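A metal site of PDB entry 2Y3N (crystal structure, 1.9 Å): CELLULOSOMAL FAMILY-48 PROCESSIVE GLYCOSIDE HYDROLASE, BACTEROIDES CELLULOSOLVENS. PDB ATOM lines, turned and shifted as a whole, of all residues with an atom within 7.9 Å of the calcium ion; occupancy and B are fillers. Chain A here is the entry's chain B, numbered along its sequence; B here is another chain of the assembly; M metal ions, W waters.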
ATOM      1  N   LEU A   5     -13.332 -13.278  -9.520  1.00  0.00           N
ATOM      2  CA  LEU A   5     -13.985 -14.340 -10.308  1.00  0.00           C
ATOM      3  C   LEU A   5     -13.273 -14.414 -11.676  1.00  0.00           C
ATOM      4  O   LEU A   5     -12.812 -13.388 -12.236  1.00  0.00           O
ATOM      5  CB  LEU A   5     -15.500 -14.077 -10.500  1.00  0.00           C
ATOM      6  CG  LEU A   5     -16.312 -13.689  -9.252  1.00  0.00           C
ATOM      7  CD1 LEU A   5     -17.669 -13.077  -9.611  1.00  0.00           C
ATOM      8  CD2 LEU A   5     -16.540 -14.907  -8.318  1.00  0.00           C
ATOM      9  N   GLY A   7     -12.741 -14.122 -15.218  1.00  0.00           N
ATOM     10  CA  GLY A   7     -13.346 -13.306 -16.267  1.00  0.00           C
ATOM     11  C   GLY A   7     -13.739 -11.915 -15.846  1.00  0.00           C
ATOM     12  O   GLY A   7     -14.028 -11.098 -16.677  1.00  0.00           O
ATOM     13  N   ASP A   8     -13.672 -11.621 -14.545  1.00  0.00           N
ATOM     14  CA  ASP A   8     -13.920 -10.278 -14.006  1.00  0.00           C
ATOM     15  C   ASP A   8     -12.729  -9.323 -14.228  1.00  0.00           C
ATOM     16  O   ASP A   8     -12.020  -8.915 -13.263  1.00  0.00           O
ATOM     17  CB  ASP A   8     -14.280 -10.357 -12.518  1.00  0.00           C
ATOM     18  CG  ASP A   8     -14.745  -9.037 -11.972  1.00  0.00           C
ATOM     19  OD1 ASP A   8     -14.947  -8.099 -12.765  1.00  0.00           O
ATOM     20  OD2 ASP A   8     -14.828  -8.912 -10.735  1.00  0.00           O
ATOM     21  N   LEU A   9     -12.551  -8.895 -15.465  1.00  0.00           N
ATOM     22  CA  LEU A   9     -11.357  -8.158 -15.822  1.00  0.00           C
ATOM     23  C   LEU A   9     -11.228  -6.773 -15.188  1.00  0.00           C
ATOM     24  O   LEU A   9     -10.117  -6.265 -15.056  1.00  0.00           O
ATOM     25  CB  LEU A   9     -11.225  -8.066 -17.350  1.00  0.00           C
ATOM     26  CG  LEU A   9     -10.533  -9.186 -18.117  1.00  0.00           C
ATOM     27  CD1 LEU A   9     -10.792 -10.495 -17.460  1.00  0.00           C
ATOM     28  CD2 LEU A   9     -10.893  -9.280 -19.611  1.00  0.00           C
ATOM     29  N   ASN A  10     -12.345  -6.126 -14.860  1.00  0.00           N
ATOM     30  CA  ASN A  10     -12.276  -4.802 -14.213  1.00  0.00           C
ATOM     31  C   ASN A  10     -12.513  -4.875 -12.702  1.00  0.00           C
ATOM     32  O   ASN A  10     -12.717  -3.845 -12.063  1.00  0.00           O
ATOM     33  CB  ASN A  10     -13.234  -3.764 -14.842  1.00  0.00           C
ATOM     34  CG  ASN A  10     -14.722  -4.216 -14.773  1.00  0.00           C
ATOM     35  OD1 ASN A  10     -15.037  -5.213 -14.084  1.00  0.00           O
ATOM     36  ND2 ASN A  10     -15.584  -3.546 -15.507  1.00  0.00           N
ATOM     37  N   GLY A  11     -12.525  -6.069 -12.121  1.00  0.00           N
ATOM     38  CA  GLY A  11     -12.602  -6.165 -10.655  1.00  0.00           C
ATOM     39  C   GLY A  11     -13.821  -5.538  -9.996  1.00  0.00           C
ATOM     40  O   GLY A  11     -13.710  -5.002  -8.871  1.00  0.00           O
ATOM     41  N   ASP A  12     -14.982  -5.592 -10.644  1.00  0.00           N
ATOM     42  CA  ASP A  12     -16.228  -5.114  -9.983  1.00  0.00           C
ATOM     43  C   ASP A  12     -17.197  -6.193  -9.417  1.00  0.00           C
ATOM     44  O   ASP A  12     -18.332  -5.883  -9.019  1.00  0.00           O
ATOM     45  CB  ASP A  12     -16.987  -4.095 -10.886  1.00  0.00           C
ATOM     46  CG  ASP A  12     -17.567  -4.752 -12.139  1.00  0.00           C
ATOM     47  OD1 ASP A  12     -17.452  -5.988 -12.214  1.00  0.00           O
ATOM     48  OD2 ASP A  12     -18.131  -4.070 -13.034  1.00  0.00           O
ATOM     49  N   GLY A  13     -16.784  -7.466  -9.366  1.00  0.00           N
ATOM     50  CA  GLY A  13     -17.653  -8.499  -8.779  1.00  0.00           C
ATOM     51  C   GLY A  13     -18.719  -9.148  -9.703  1.00  0.00           C
ATOM     52  O   GLY A  13     -19.461 -10.054  -9.267  1.00  0.00           O
ATOM     53  N   VAL A  14     -18.806  -8.706 -10.974  1.00  0.00           N
ATOM     54  CA  VAL A  14     -19.784  -9.241 -11.949  1.00  0.00           C
ATOM     55  C   VAL A  14     -19.051  -9.536 -13.314  1.00  0.00           C
ATOM     56  O   VAL A  14     -17.964  -9.012 -13.594  1.00  0.00           O
ATOM     57  CB  VAL A  14     -21.086  -8.297 -12.078  1.00  0.00           C
ATOM     58  CG1 VAL A  14     -21.654  -7.922 -10.669  1.00  0.00           C
ATOM     59  CG2 VAL A  14     -20.765  -6.978 -12.790  1.00  0.00           C
ATOM     60  N   ILE A  15     -19.608 -10.423 -14.129  1.00  0.00           N
ATOM     61  CA  ILE A  15     -19.033 -10.697 -15.432  1.00  0.00           C
ATOM     62  C   ILE A  15     -20.066 -10.206 -16.469  1.00  0.00           C
ATOM     63  O   ILE A  15     -21.179 -10.770 -16.614  1.00  0.00           O
ATOM     64  CB  ILE A  15     -18.670 -12.173 -15.611  1.00  0.00           C
ATOM     65  CG1 ILE A  15     -17.806 -12.740 -14.458  1.00  0.00           C
ATOM     66  CG2 ILE A  15     -18.085 -12.503 -17.059  1.00  0.00           C
ATOM     67  CD1 ILE A  15     -16.674 -11.969 -14.089  1.00  0.00           C
ATOM     68  N   ASN A  16     -19.693  -9.113 -17.171  1.00  0.00           N
ATOM     69  CA  ASN A  16     -20.594  -8.513 -18.149  1.00  0.00           C
ATOM     70  C   ASN A  16     -19.824  -7.941 -19.347  1.00  0.00           C
ATOM     71  O   ASN A  16     -18.571  -8.023 -19.385  1.00  0.00           O
ATOM     72  CB  ASN A  16     -21.543  -7.487 -17.509  1.00  0.00           C
ATOM     73  CG  ASN A  16     -20.811  -6.278 -16.955  1.00  0.00           C
ATOM     74  OD1 ASN A  16     -19.698  -5.956 -17.396  1.00  0.00           O
ATOM     75  ND2 ASN A  16     -21.448  -5.582 -16.011  1.00  0.00           N
ATOM     76  N   MET A  17     -20.534  -7.303 -20.261  1.00  0.00           N
ATOM     77  CA  MET A  17     -19.905  -6.796 -21.486  1.00  0.00           C
ATOM     78  C   MET A  17     -18.699  -5.871 -21.167  1.00  0.00           C
ATOM     79  O   MET A  17     -17.834  -5.695 -22.007  1.00  0.00           O
ATOM     80  CB  MET A  17     -20.901  -6.114 -22.374  1.00  0.00           C
ATOM     81  CG  MET A  17     -20.405  -5.792 -23.781  1.00  0.00           C
ATOM     82  SD  MET A  17     -19.884  -7.263 -24.703  1.00  0.00           S
ATOM     83  CE  MET A  17     -21.462  -7.941 -25.310  1.00  0.00           C
ATOM     84  N   ALA A  18     -18.648  -5.289 -19.972  1.00  0.00           N
ATOM     85  CA  ALA A  18     -17.540  -4.354 -19.660  1.00  0.00           C
ATOM     86  C   ALA A  18     -16.246  -5.168 -19.595  1.00  0.00           C
ATOM     87  O   ALA A  18     -15.182  -4.692 -20.002  1.00  0.00           O
ATOM     88  CB  ALA A  18     -17.798  -3.534 -18.352  1.00  0.00           C
ATOM     89  N   ASP A  19     -16.332  -6.385 -19.065  1.00  0.00           N
ATOM     90  CA  ASP A  19     -15.188  -7.275 -19.052  1.00  0.00           C
ATOM     91  C   ASP A  19     -14.769  -7.722 -20.448  1.00  0.00           C
ATOM     92  O   ASP A  19     -13.599  -7.750 -20.767  1.00  0.00           O
ATOM     93  CB  ASP A  19     -15.498  -8.462 -18.201  1.00  0.00           C
ATOM     94  CG  ASP A  19     -15.900  -8.071 -16.809  1.00  0.00           C
ATOM     95  OD1 ASP A  19     -15.049  -7.516 -16.071  1.00  0.00           O
ATOM     96  OD2 ASP A  19     -17.075  -8.297 -16.476  1.00  0.00           O
ATOM     97  N   VAL A  20     -15.754  -8.089 -21.252  1.00  0.00           N
ATOM     98  CA  VAL A  20     -15.511  -8.463 -22.664  1.00  0.00           C
ATOM     99  C   VAL A  20     -14.817  -7.338 -23.488  1.00  0.00           C
ATOM    100  O   VAL A  20     -13.916  -7.596 -24.332  1.00  0.00           O
ATOM    101  CB  VAL A  20     -16.892  -8.835 -23.355  1.00  0.00           C
ATOM    102  CG1 VAL A  20     -16.627  -9.370 -24.727  1.00  0.00           C
ATOM    103  CG2 VAL A  20     -17.637  -9.848 -22.509  1.00  0.00           C
ATOM    104  N   ILE A  22     -12.724  -5.154 -22.331  1.00  0.00           N
ATOM    105  CA  ILE A  22     -11.266  -5.075 -22.021  1.00  0.00           C
ATOM    106  C   ILE A  22     -10.536  -6.163 -22.818  1.00  0.00           C
ATOM    107  O   ILE A  22      -9.422  -5.974 -23.336  1.00  0.00           O
ATOM    108  CB  ILE A  22     -11.011  -5.224 -20.536  1.00  0.00           C
ATOM    109  CG1 ILE A  22     -11.684  -4.062 -19.791  1.00  0.00           C
ATOM    110  CG2 ILE A  22      -9.502  -5.289 -20.223  1.00  0.00           C
ATOM    111  CD1 ILE A  22     -11.878  -4.330 -18.341  1.00  0.00           C
ATOM    112  N   LEU A  56     -14.589 -16.420 -20.910  1.00  0.00           N
ATOM    113  CA  LEU A  56     -15.448 -15.348 -20.449  1.00  0.00           C
ATOM    114  C   LEU A  56     -16.957 -15.633 -20.684  1.00  0.00           C
ATOM    115  O   LEU A  56     -17.770 -15.447 -19.763  1.00  0.00           O
ATOM    116  CB  LEU A  56     -15.077 -14.036 -21.169  1.00  0.00           C
ATOM    117  CG  LEU A  56     -15.164 -12.766 -20.346  1.00  0.00           C
ATOM    118  CD1 LEU A  56     -14.505 -13.007 -19.047  1.00  0.00           C
ATOM    119  CD2 LEU A  56     -14.450 -11.659 -21.034  1.00  0.00           C
ATOM    120  N   LYS A  62     -22.349 -14.048 -14.192  1.00  0.00           N
ATOM    121  CA  LYS A  62     -21.968 -14.397 -12.801  1.00  0.00           C
ATOM    122  C   LYS A  62     -21.671 -13.167 -11.953  1.00  0.00           C
ATOM    123  O   LYS A  62     -21.149 -12.172 -12.497  1.00  0.00           O
ATOM    124  CB  LYS A  62     -20.753 -15.295 -12.770  1.00  0.00           C
ATOM    125  CG  LYS A  62     -21.005 -16.742 -13.052  1.00  0.00           C
ATOM    126  CD  LYS A  62     -19.745 -17.472 -12.712  1.00  0.00           C
ATOM    127  CE  LYS A  62     -19.375 -17.188 -11.276  1.00  0.00           C
ATOM    128  NZ  LYS A  62     -18.042 -17.771 -10.939  1.00  0.00           N
ATOM    129  N   SER B 139     -26.191  -8.982 -12.880  1.00  0.00           N
ATOM    130  CA  SER B 139     -24.857  -8.729 -13.394  1.00  0.00           C
ATOM    131  C   SER B 139     -24.604  -7.363 -14.000  1.00  0.00           C
ATOM    132  O   SER B 139     -23.534  -7.121 -14.569  1.00  0.00           O
ATOM    133  CB  SER B 139     -24.488  -9.805 -14.346  1.00  0.00           C
ATOM    134  OG  SER B 139     -25.085  -9.582 -15.568  1.00  0.00           O
ATOM    135  N   ASN B 141     -24.264  -3.993 -12.583  1.00  0.00           N
ATOM    136  CA  ASN B 141     -24.086  -3.227 -11.348  1.00  0.00           C
ATOM    137  C   ASN B 141     -24.075  -1.698 -11.525  1.00  0.00           C
ATOM    138  O   ASN B 141     -24.673  -0.982 -10.726  1.00  0.00           O
ATOM    139  CB  ASN B 141     -22.848  -3.740 -10.552  1.00  0.00           C
ATOM    140  CG  ASN B 141     -21.516  -3.498 -11.278  1.00  0.00           C
ATOM    141  OD1 ASN B 141     -21.451  -3.360 -12.507  1.00  0.00           O
ATOM    142  ND2 ASN B 141     -20.425  -3.460 -10.492  1.00  0.00           N
HETATM  143 CA    CA M   1     -16.592  -7.162 -14.280  1.00  0.00          CA
HETATM  144  O   HOH W   1     -18.065  -5.390 -15.251  1.00  0.00           O
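Within 4 Å of the calcium ion: Asp 8, Asn 10, Asp 12, Val 14 and Asp 19.
The calcium ion is bound by OD1 of Asp 19, O of Val 14, OD1 of Asp 8, water W1, OD1 of Asn 10, OD2 of Asp 19 and OD1 of Asp 12. The calcium ion has seven donor atoms within binding distance.
Water W1 lies within hydrogen-bond range of OD2 of Asp 12, OD1 of Asn 16 and ND2 of Asn 10.
OD1 of Asp 8 lies close to N of Gly 11, 3.2 Å away. N of Leu 9 lies close to OD1 of Asp 19, at 2.9 Å. The backbone NH (N) of Asn 16 sits close to the side-chain carboxylate (OD2) of Asp 19 (2.8 Å). The side-chain amide oxygen (OD1) of Asn 141 of chain B lies close to the side-chain carboxylate (OD2) of Asp 12 (3.4 Å). OD2 of Asp 8 lies within hydrogen-bond range of N of Gly 13 (2.8 Å).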
